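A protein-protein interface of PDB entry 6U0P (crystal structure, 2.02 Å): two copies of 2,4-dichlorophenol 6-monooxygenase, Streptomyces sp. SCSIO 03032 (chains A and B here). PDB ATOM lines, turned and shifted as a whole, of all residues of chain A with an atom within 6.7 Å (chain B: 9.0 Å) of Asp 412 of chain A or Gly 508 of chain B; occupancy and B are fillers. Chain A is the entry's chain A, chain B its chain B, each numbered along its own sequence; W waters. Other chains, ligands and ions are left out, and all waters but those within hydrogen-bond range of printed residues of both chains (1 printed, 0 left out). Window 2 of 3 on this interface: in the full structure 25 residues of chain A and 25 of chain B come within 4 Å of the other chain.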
ATOM      1  N   THR A 408       0.798  27.725 -25.612  1.00  0.00           N
ATOM      2  CA  THR A 408       1.767  26.599 -25.618  1.00  0.00           C
ATOM      3  C   THR A 408       3.135  27.034 -26.152  1.00  0.00           C
ATOM      4  O   THR A 408       4.026  26.157 -26.289  1.00  0.00           O
ATOM      5  CB  THR A 408       1.233  25.447 -26.469  1.00  0.00           C
ATOM      6  OG1 THR A 408       1.170  25.931 -27.817  1.00  0.00           O
ATOM      7  CG2 THR A 408      -0.112  24.958 -25.970  1.00  0.00           C
ATOM      8  N   LEU A 409       3.312  28.315 -26.471  1.00  0.00           N
ATOM      9  CA  LEU A 409       4.630  28.850 -26.901  1.00  0.00           C
ATOM     10  C   LEU A 409       5.654  28.729 -25.751  1.00  0.00           C
ATOM     11  O   LEU A 409       6.845  28.553 -26.071  1.00  0.00           O
ATOM     12  CB  LEU A 409       4.483  30.308 -27.355  1.00  0.00           C
ATOM     13  CG  LEU A 409       5.783  31.009 -27.773  1.00  0.00           C
ATOM     14  CD1 LEU A 409       6.329  30.395 -29.034  1.00  0.00           C
ATOM     15  CD2 LEU A 409       5.614  32.520 -27.951  1.00  0.00           C
ATOM     16  N   HIS A 410       5.232  28.839 -24.481  1.00  0.00           N
ATOM     17  CA  HIS A 410       6.127  28.830 -23.281  1.00  0.00           C
ATOM     18  C   HIS A 410       6.183  27.443 -22.625  1.00  0.00           C
ATOM     19  O   HIS A 410       6.614  27.357 -21.461  1.00  0.00           O
ATOM     20  CB  HIS A 410       5.680  29.899 -22.272  1.00  0.00           C
ATOM     21  CG  HIS A 410       5.631  31.273 -22.857  1.00  0.00           C
ATOM     22  ND1 HIS A 410       6.276  31.599 -24.041  1.00  0.00           N
ATOM     23  CD2 HIS A 410       5.036  32.406 -22.431  1.00  0.00           C
ATOM     24  CE1 HIS A 410       6.068  32.865 -24.323  1.00  0.00           C
ATOM     25  NE2 HIS A 410       5.310  33.384 -23.350  1.00  0.00           N
ATOM     26  N   GLU A 411       5.756  26.392 -23.320  1.00  0.00           N
ATOM     27  CA  GLU A 411       5.843  25.005 -22.794  1.00  0.00           C
ATOM     28  C   GLU A 411       7.258  24.457 -23.000  1.00  0.00           C
ATOM     29  O   GLU A 411       7.963  24.881 -23.956  1.00  0.00           O
ATOM     30  CB  GLU A 411       4.819  24.079 -23.444  1.00  0.00           C
ATOM     31  CG  GLU A 411       3.445  24.242 -22.843  1.00  0.00           C
ATOM     32  CD  GLU A 411       2.413  23.294 -23.402  1.00  0.00           C
ATOM     33  OE1 GLU A 411       2.679  22.660 -24.466  1.00  0.00           O
ATOM     34  OE2 GLU A 411       1.351  23.191 -22.772  1.00  0.00           O
ATOM     35  N   ASP A 412       7.635  23.577 -22.071  1.00  0.00           N
ATOM     36  CA  ASP A 412       8.869  22.754 -22.048  1.00  0.00           C
ATOM     37  C   ASP A 412       8.679  21.598 -23.037  1.00  0.00           C
ATOM     38  O   ASP A 412       8.311  20.478 -22.594  1.00  0.00           O
ATOM     39  CB  ASP A 412       9.103  22.251 -20.615  1.00  0.00           C
ATOM     40  CG  ASP A 412      10.359  21.416 -20.423  1.00  0.00           C
ATOM     41  OD1 ASP A 412      11.387  21.769 -21.039  1.00  0.00           O
ATOM     42  OD2 ASP A 412      10.294  20.424 -19.652  1.00  0.00           O
ATOM     43  N   THR A 413       8.832  21.865 -24.331  1.00  0.00           N
ATOM     44  CA  THR A 413       8.753  20.823 -25.393  1.00  0.00           C
ATOM     45  C   THR A 413       9.639  21.252 -26.553  1.00  0.00           C
ATOM     46  O   THR A 413      10.000  22.471 -26.623  1.00  0.00           O
ATOM     47  CB  THR A 413       7.317  20.585 -25.891  1.00  0.00           C
ATOM     48  OG1 THR A 413       6.823  21.778 -26.510  1.00  0.00           O
ATOM     49  CG2 THR A 413       6.354  20.174 -24.800  1.00  0.00           C
ATOM     50  N   GLU A 414       9.937  20.308 -27.440  1.00  0.00           N
ATOM     51  CA  GLU A 414      10.775  20.555 -28.633  1.00  0.00           C
ATOM     52  C   GLU A 414      10.103  21.604 -29.512  1.00  0.00           C
ATOM     53  O   GLU A 414      10.811  22.536 -29.916  1.00  0.00           O
ATOM     54  CB  GLU A 414      11.015  19.274 -29.437  1.00  0.00           C
ATOM     55  CG  GLU A 414      12.074  19.428 -30.525  1.00  0.00           C
ATOM     56  CD  GLU A 414      13.368  20.152 -30.142  1.00  0.00           C
ATOM     57  OE1 GLU A 414      14.004  20.732 -31.055  1.00  0.00           O
ATOM     58  OE2 GLU A 414      13.752  20.150 -28.940  1.00  0.00           O
ATOM     59  N   ALA A 416       7.690  24.004 -29.008  1.00  0.00           N
ATOM     60  CA  ALA A 416       7.702  25.330 -28.345  1.00  0.00           C
ATOM     61  C   ALA A 416       9.111  25.960 -28.362  1.00  0.00           C
ATOM     62  O   ALA A 416       9.199  27.168 -28.728  1.00  0.00           O
ATOM     63  CB  ALA A 416       7.148  25.193 -26.947  1.00  0.00           C
ATOM     64  N   ARG A 417      10.167  25.201 -28.007  1.00  0.00           N
ATOM     65  CA  ARG A 417      11.589  25.659 -28.064  1.00  0.00           C
ATOM     66  C   ARG A 417      11.947  26.120 -29.487  1.00  0.00           C
ATOM     67  O   ARG A 417      12.589  27.208 -29.594  1.00  0.00           O
ATOM     68  CB  ARG A 417      12.581  24.585 -27.594  1.00  0.00           C
ATOM     69  CG  ARG A 417      12.858  24.619 -26.095  1.00  0.00           C
ATOM     70  CD  ARG A 417      13.920  23.645 -25.580  1.00  0.00           C
ATOM     71  NE  ARG A 417      13.733  22.276 -26.051  1.00  0.00           N
ATOM     72  CZ  ARG A 417      12.937  21.350 -25.505  1.00  0.00           C
ATOM     73  NH1 ARG A 417      12.195  21.600 -24.438  1.00  0.00           N
ATOM     74  NH2 ARG A 417      12.869  20.154 -26.064  1.00  0.00           N
ATOM     75  N   ARG A 420       9.870  29.360 -30.417  1.00  0.00           N
ATOM     76  CA  ARG A 420      10.566  30.353 -29.559  1.00  0.00           C
ATOM     77  C   ARG A 420      11.774  30.918 -30.312  1.00  0.00           C
ATOM     78  O   ARG A 420      12.052  32.173 -30.185  1.00  0.00           O
ATOM     79  CB  ARG A 420      10.980  29.699 -28.237  1.00  0.00           C
ATOM     80  CG  ARG A 420      10.662  30.515 -26.995  1.00  0.00           C
ATOM     81  CD  ARG A 420       9.872  29.698 -25.992  1.00  0.00           C
ATOM     82  NE  ARG A 420      10.639  28.619 -25.372  1.00  0.00           N
ATOM     83  CZ  ARG A 420      10.114  27.560 -24.759  1.00  0.00           C
ATOM     84  NH1 ARG A 420       8.800  27.386 -24.698  1.00  0.00           N
ATOM     85  NH2 ARG A 420      10.912  26.656 -24.220  1.00  0.00           N
ATOM     86  N   THR B 505      13.042  30.578 -11.590  1.00  0.00           N
ATOM     87  CA  THR B 505      13.031  29.390 -12.486  1.00  0.00           C
ATOM     88  C   THR B 505      12.439  29.793 -13.833  1.00  0.00           C
ATOM     89  O   THR B 505      12.223  31.004 -14.064  1.00  0.00           O
ATOM     90  CB  THR B 505      12.285  28.236 -11.806  1.00  0.00           C
ATOM     91  OG1 THR B 505      10.911  28.577 -11.587  1.00  0.00           O
ATOM     92  CG2 THR B 505      12.856  27.915 -10.446  1.00  0.00           C
ATOM     93  N   GLY B 506      12.179  28.807 -14.689  1.00  0.00           N
ATOM     94  CA  GLY B 506      11.736  28.996 -16.079  1.00  0.00           C
ATOM     95  C   GLY B 506      10.998  27.765 -16.588  1.00  0.00           C
ATOM     96  O   GLY B 506      10.665  26.867 -15.819  1.00  0.00           O
ATOM     97  N   PRO B 507      10.749  27.684 -17.909  1.00  0.00           N
ATOM     98  CA  PRO B 507      10.082  26.526 -18.502  1.00  0.00           C
ATOM     99  C   PRO B 507      10.837  25.236 -18.156  1.00  0.00           C
ATOM    100  O   PRO B 507      12.058  25.209 -18.278  1.00  0.00           O
ATOM    101  CB  PRO B 507      10.154  26.787 -20.020  1.00  0.00           C
ATOM    102  CG  PRO B 507      10.356  28.281 -20.159  1.00  0.00           C
ATOM    103  CD  PRO B 507      11.126  28.693 -18.915  1.00  0.00           C
ATOM    104  N   GLY B 508      10.106  24.212 -17.729  1.00  0.00           N
ATOM    105  CA  GLY B 508      10.677  22.910 -17.332  1.00  0.00           C
ATOM    106  C   GLY B 508      11.239  22.935 -15.918  1.00  0.00           C
ATOM    107  O   GLY B 508      11.836  21.933 -15.524  1.00  0.00           O
ATOM    108  N   GLY B 509      10.978  23.999 -15.154  1.00  0.00           N
ATOM    109  CA  GLY B 509      11.426  24.143 -13.756  1.00  0.00           C
ATOM    110  C   GLY B 509      10.511  23.550 -12.699  1.00  0.00           C
ATOM    111  O   GLY B 509      10.801  23.793 -11.512  1.00  0.00           O
ATOM    112  N   GLU B 510       9.464  22.793 -13.042  1.00  0.00           N
ATOM    113  CA  GLU B 510       8.474  22.265 -12.043  1.00  0.00           C
ATOM    114  C   GLU B 510       9.168  21.466 -10.929  1.00  0.00           C
ATOM    115  O   GLU B 510       8.730  21.520  -9.773  1.00  0.00           O
ATOM    116  CB  GLU B 510       7.396  21.400 -12.710  1.00  0.00           C
ATOM    117  CG  GLU B 510       6.449  22.182 -13.620  1.00  0.00           C
ATOM    118  CD  GLU B 510       6.990  22.564 -14.997  1.00  0.00           C
ATOM    119  OE1 GLU B 510       8.086  22.061 -15.414  1.00  0.00           O
ATOM    120  OE2 GLU B 510       6.311  23.364 -15.670  1.00  0.00           O
ATOM    121  N   PRO B 511      10.238  20.678 -11.201  1.00  0.00           N
ATOM    122  CA  PRO B 511      10.884  19.900 -10.140  1.00  0.00           C
ATOM    123  C   PRO B 511      11.358  20.746  -8.958  1.00  0.00           C
ATOM    124  O   PRO B 511      11.437  20.206  -7.903  1.00  0.00           O
ATOM    125  CB  PRO B 511      12.071  19.209 -10.828  1.00  0.00           C
ATOM    126  CG  PRO B 511      11.597  19.066 -12.263  1.00  0.00           C
ATOM    127  CD  PRO B 511      10.799  20.338 -12.525  1.00  0.00           C
ATOM    128  N   TRP B 512      11.621  22.036  -9.161  1.00  0.00           N
ATOM    129  CA  TRP B 512      12.059  22.976  -8.086  1.00  0.00           C
ATOM    130  C   TRP B 512      10.953  23.186  -7.043  1.00  0.00           C
ATOM    131  O   TRP B 512      11.291  23.544  -5.915  1.00  0.00           O
ATOM    132  CB  TRP B 512      12.476  24.317  -8.695  1.00  0.00           C
ATOM    133  CG  TRP B 512      13.715  24.184  -9.513  1.00  0.00           C
ATOM    134  CD1 TRP B 512      13.821  24.264 -10.866  1.00  0.00           C
ATOM    135  CD2 TRP B 512      15.047  23.943  -9.019  1.00  0.00           C
ATOM    136  NE1 TRP B 512      15.127  24.094 -11.247  1.00  0.00           N
ATOM    137  CE2 TRP B 512      15.901  23.887 -10.140  1.00  0.00           C
ATOM    138  CE3 TRP B 512      15.607  23.811  -7.746  1.00  0.00           C
ATOM    139  CZ2 TRP B 512      17.280  23.678 -10.027  1.00  0.00           C
ATOM    140  CZ3 TRP B 512      16.967  23.590  -7.633  1.00  0.00           C
ATOM    141  CH2 TRP B 512      17.791  23.527  -8.756  1.00  0.00           C
ATOM    142  N   ARG B 513       9.684  22.955  -7.399  1.00  0.00           N
ATOM    143  CA  ARG B 513       8.530  23.056  -6.452  1.00  0.00           C
ATOM    144  C   ARG B 513       8.705  22.086  -5.280  1.00  0.00           C
ATOM    145  O   ARG B 513       8.736  22.543  -4.129  1.00  0.00           O
ATOM    146  CB  ARG B 513       7.192  22.693  -7.114  1.00  0.00           C
ATOM    147  CG  ARG B 513       6.271  23.875  -7.358  1.00  0.00           C
ATOM    148  CD  ARG B 513       6.775  24.695  -8.530  1.00  0.00           C
ATOM    149  NE  ARG B 513       5.963  25.870  -8.845  1.00  0.00           N
ATOM    150  CZ  ARG B 513       5.806  26.364 -10.067  1.00  0.00           C
ATOM    151  NH1 ARG B 513       6.356  25.768 -11.113  1.00  0.00           N
ATOM    152  NH2 ARG B 513       5.071  27.446 -10.253  1.00  0.00           N
ATOM    153  N   PRO B 531       8.508  31.392 -11.148  1.00  0.00           N
ATOM    154  CA  PRO B 531       8.804  31.109 -12.551  1.00  0.00           C
ATOM    155  C   PRO B 531       8.737  32.391 -13.381  1.00  0.00           C
ATOM    156  O   PRO B 531       7.782  33.122 -13.186  1.00  0.00           O
ATOM    157  CB  PRO B 531       7.699  30.130 -12.976  1.00  0.00           C
ATOM    158  CG  PRO B 531       6.561  30.455 -12.031  1.00  0.00           C
ATOM    159  CD  PRO B 531       7.225  30.807 -10.713  1.00  0.00           C
ATOM    160  N   ILE B 532       9.717  32.613 -14.258  1.00  0.00           N
ATOM    161  CA  ILE B 532       9.736  33.756 -15.218  1.00  0.00           C
ATOM    162  C   ILE B 532       9.575  33.203 -16.629  1.00  0.00           C
ATOM    163  O   ILE B 532      10.448  32.414 -17.025  1.00  0.00           O
ATOM    164  CB  ILE B 532      11.018  34.578 -15.081  1.00  0.00           C
ATOM    165  CG1 ILE B 532      11.127  35.160 -13.679  1.00  0.00           C
ATOM    166  CG2 ILE B 532      11.089  35.667 -16.137  1.00  0.00           C
ATOM    167  CD1 ILE B 532      12.442  35.842 -13.448  1.00  0.00           C
ATOM    168  N   GLY B 533       8.505  33.593 -17.330  1.00  0.00           N
ATOM    169  CA  GLY B 533       8.245  33.192 -18.722  1.00  0.00           C
ATOM    170  C   GLY B 533       7.720  31.775 -18.788  1.00  0.00           C
ATOM    171  O   GLY B 533       8.004  31.082 -19.764  1.00  0.00           O
ATOM    172  N   ALA B 534       7.024  31.347 -17.737  1.00  0.00           N
ATOM    173  CA  ALA B 534       6.477  29.985 -17.552  1.00  0.00           C
ATOM    174  C   ALA B 534       5.418  30.038 -16.457  1.00  0.00           C
ATOM    175  O   ALA B 534       5.524  30.921 -15.566  1.00  0.00           O
ATOM    176  CB  ALA B 534       7.559  28.986 -17.160  1.00  0.00           C
ATOM    177  N   GLY B 535       4.462  29.113 -16.496  1.00  0.00           N
ATOM    178  CA  GLY B 535       3.534  28.863 -15.368  1.00  0.00           C
ATOM    179  C   GLY B 535       2.691  30.085 -14.972  1.00  0.00           C
ATOM    180  O   GLY B 535       2.282  30.127 -13.761  1.00  0.00           O
ATOM    181  N   ARG B 549      20.728  35.329 -17.006  1.00  0.00           N
ATOM    182  CA  ARG B 549      20.556  34.413 -15.861  1.00  0.00           C
ATOM    183  C   ARG B 549      21.673  33.342 -15.831  1.00  0.00           C
ATOM    184  O   ARG B 549      21.869  32.760 -14.778  1.00  0.00           O
ATOM    185  CB  ARG B 549      19.149  33.804 -15.878  1.00  0.00           C
ATOM    186  CG  ARG B 549      18.901  32.773 -16.961  1.00  0.00           C
ATOM    187  CD  ARG B 549      17.471  32.271 -16.867  1.00  0.00           C
ATOM    188  NE  ARG B 549      17.021  31.668 -18.112  1.00  0.00           N
ATOM    189  CZ  ARG B 549      15.744  31.561 -18.482  1.00  0.00           C
ATOM    190  NH1 ARG B 549      14.766  31.914 -17.661  1.00  0.00           N
ATOM    191  NH2 ARG B 549      15.456  31.023 -19.645  1.00  0.00           N
ATOM    192  N   GLU B 552      20.173  27.367 -17.637  1.00  0.00           N
ATOM    193  CA  GLU B 552      19.213  26.975 -18.682  1.00  0.00           C
ATOM    194  C   GLU B 552      17.793  27.282 -18.194  1.00  0.00           C
ATOM    195  O   GLU B 552      17.621  27.540 -16.983  1.00  0.00           O
ATOM    196  CB  GLU B 552      19.346  25.485 -18.969  1.00  0.00           C
ATOM    197  CG  GLU B 552      20.679  25.065 -19.515  1.00  0.00           C
ATOM    198  CD  GLU B 552      20.441  23.839 -20.383  1.00  0.00           C
ATOM    199  OE1 GLU B 552      19.927  22.787 -19.855  1.00  0.00           O
ATOM    200  OE2 GLU B 552      20.649  23.967 -21.609  1.00  0.00           O
ATOM    201  N   GLU B 553      16.814  27.236 -19.108  1.00  0.00           N
ATOM    202  CA  GLU B 553      15.365  27.418 -18.823  1.00  0.00           C
ATOM    203  C   GLU B 553      14.950  26.644 -17.556  1.00  0.00           C
ATOM    204  O   GLU B 553      14.140  27.157 -16.776  1.00  0.00           O
ATOM    205  CB  GLU B 553      14.526  26.835 -19.961  1.00  0.00           C
ATOM    206  CG  GLU B 553      14.512  27.653 -21.224  1.00  0.00           C
ATOM    207  CD  GLU B 553      13.585  27.078 -22.282  1.00  0.00           C
ATOM    208  OE1 GLU B 553      13.550  25.830 -22.443  1.00  0.00           O
ATOM    209  OE2 GLU B 553      12.879  27.876 -22.924  1.00  0.00           O
ATOM    210  N   SER B 554      15.383  25.391 -17.415  1.00  0.00           N
ATOM    211  CA  SER B 554      14.910  24.469 -16.343  1.00  0.00           C
ATOM    212  C   SER B 554      15.759  24.651 -15.066  1.00  0.00           C
ATOM    213  O   SER B 554      15.438  24.017 -14.049  1.00  0.00           O
ATOM    214  CB  SER B 554      14.940  23.028 -16.822  1.00  0.00           C
ATOM    215  OG  SER B 554      16.268  22.511 -16.744  1.00  0.00           O
ATOM    216  N   GLY B 555      16.750  25.539 -15.094  1.00  0.00           N
ATOM    217  CA  GLY B 555      17.665  25.782 -13.963  1.00  0.00           C
ATOM    218  C   GLY B 555      17.063  26.727 -12.925  1.00  0.00           C
ATOM    219  O   GLY B 555      15.821  26.959 -12.935  1.00  0.00           O
ATOM    220  N   ALA B 556      17.892  27.264 -12.034  1.00  0.00           N
ATOM    221  CA  ALA B 556      17.397  28.055 -10.883  1.00  0.00           C
ATOM    222  C   ALA B 556      18.475  28.997 -10.390  1.00  0.00           C
ATOM    223  O   ALA B 556      19.673  28.657 -10.476  1.00  0.00           O
ATOM    224  CB  ALA B 556      16.932  27.137  -9.787  1.00  0.00           C
ATOM    225  N   ASP B 571      20.405  23.365 -14.452  1.00  0.00           N
ATOM    226  CA  ASP B 571      19.210  22.670 -14.967  1.00  0.00           C
ATOM    227  C   ASP B 571      18.509  22.016 -13.792  1.00  0.00           C
ATOM    228  O   ASP B 571      19.094  22.013 -12.683  1.00  0.00           O
ATOM    229  CB  ASP B 571      19.580  21.674 -16.083  1.00  0.00           C
ATOM    230  CG  ASP B 571      20.582  20.624 -15.615  1.00  0.00           C
ATOM    231  OD1 ASP B 571      20.274  19.904 -14.629  1.00  0.00           O
ATOM    232  OD2 ASP B 571      21.699  20.604 -16.158  1.00  0.00           O
ATOM    233  N   HIS B 572      17.348  21.404 -14.053  1.00  0.00           N
ATOM    234  CA  HIS B 572      16.461  20.827 -13.008  1.00  0.00           C
ATOM    235  C   HIS B 572      17.034  19.535 -12.399  1.00  0.00           C
ATOM    236  O   HIS B 572      16.523  19.118 -11.345  1.00  0.00           O
ATOM    237  CB  HIS B 572      15.052  20.589 -13.539  1.00  0.00           C
ATOM    238  CG  HIS B 572      14.972  19.455 -14.498  1.00  0.00           C
ATOM    239  ND1 HIS B 572      14.846  18.131 -14.087  1.00  0.00           N
ATOM    240  CD2 HIS B 572      15.002  19.440 -15.841  1.00  0.00           C
ATOM    241  CE1 HIS B 572      14.804  17.357 -15.147  1.00  0.00           C
ATOM    242  NE2 HIS B 572      14.902  18.135 -16.231  1.00  0.00           N
ATOM    243  N   GLY B 573      18.044  18.928 -13.009  1.00  0.00           N
ATOM    244  CA  GLY B 573      18.741  17.763 -12.424  1.00  0.00           C
ATOM    245  C   GLY B 573      19.388  18.093 -11.086  1.00  0.00           C
ATOM    246  O   GLY B 573      19.572  17.187 -10.280  1.00  0.00           O
ATOM    247  N   ALA B 575      17.928  19.781  -8.721  1.00  0.00           N
ATOM    248  CA  ALA B 575      16.800  20.124  -7.812  1.00  0.00           C
ATOM    249  C   ALA B 575      17.022  19.480  -6.439  1.00  0.00           C
ATOM    250  O   ALA B 575      16.971  20.191  -5.418  1.00  0.00           O
ATOM    251  CB  ALA B 575      15.473  19.680  -8.399  1.00  0.00           C
HETATM  252  O   HOH W   1      11.899  23.910 -22.607  1.00  0.00           O
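Gly 508 of chain B touches one residue of chain A.
No residue of chain B comes within 4 Å of Thr 413 of chain A.
Of the printed residues of chain B, Arg 417 of chain A touches Glu 553 (3.8 Å).
Printed residues of chain A within 4 Å of Gly 533 of chain B: His 410.
Printed residues of chain B within 4 Å of His 410 of chain A: Pro 507 and Gly 533.
Trp 512 of chain B touches none of the printed residues of chain A.
The nearest residue of chain B that does not touch Asp 412 of chain A is Pro 507 of chain B (4.2 Å).
The nearest printed residue of chain B that does not touch Arg 420 of chain A is Pro 507 of chain B (4.3 Å).
No position is printed for both chains.
Of the 5 pairs that touch across the chains among the printed residues, none has its exchanged pair printed and touching as well.
The guanidinium group (NH2) of Arg 420 of chain A is in salt-bridge range of the side-chain carboxylate (OE2) of Glu 553 of chain B (2.7 Å).
O of Leu 409 of chain A sits at hydrogen-bond distance from NH1 of Arg 420 of chain A, 2.7 Å away.
The side-chain carboxylate (OD1) of Asp 412 of chain A is in salt-bridge range of the guanidinium group (NH1) of Arg 417 of chain A (3.5 Å).
The backbone carbonyl oxygen of Thr 413 of chain A sits at hydrogen-bond distance from the guanidinium group of Arg 417 of chain A (3.2 Å).
The side-chain carboxylate (OE2) of Glu 414 of chain A lies within salt-bridge range of the guanidinium group (NH2) of Arg 417 of chain A, at 3.0 Å.
The backbone carbonyl oxygen (O) of Glu 553 of chain B lies close to the backbone NH (N) of Gly 506 of chain B (3.3 Å).
The backbone carbonyl oxygen of Pro 507 of chain B sits at hydrogen-bond distance from the backbone NH of Ser 554 of chain B, 3.4 Å away.
Among the printed residues, pairs that only touch across the chains: Asp 412 of chain A with Gly 508 of chain B, His 410 of chain A with Gly 533 of chain B, Arg 417 of chain A with Glu 553 of chain B and His 410 of chain A with Pro 507 of chain B.
Water W1 lies within hydrogen-bond range of OE1 of Glu 553 of chain B (2.5 Å), OD1 of Asp 412 of chain A (2.7 Å), NH1 of Arg 417 of chain A (3.0 Å) and NH2 of Arg 420 of chain A (3.3 Å).
Hydrophobic or aromatic side chains of chain A within 4 Å of the printed part of chain B: His 410.
Along chain A the printed residues that touch a printed residue of chain B span positions 410 to 420.
Among the printed residues, Asp or Glu carboxylates within 4 Å of a Lys or Arg side-chain nitrogen of the other chain: Arg 420 of chain A with Glu 553 of chain B.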
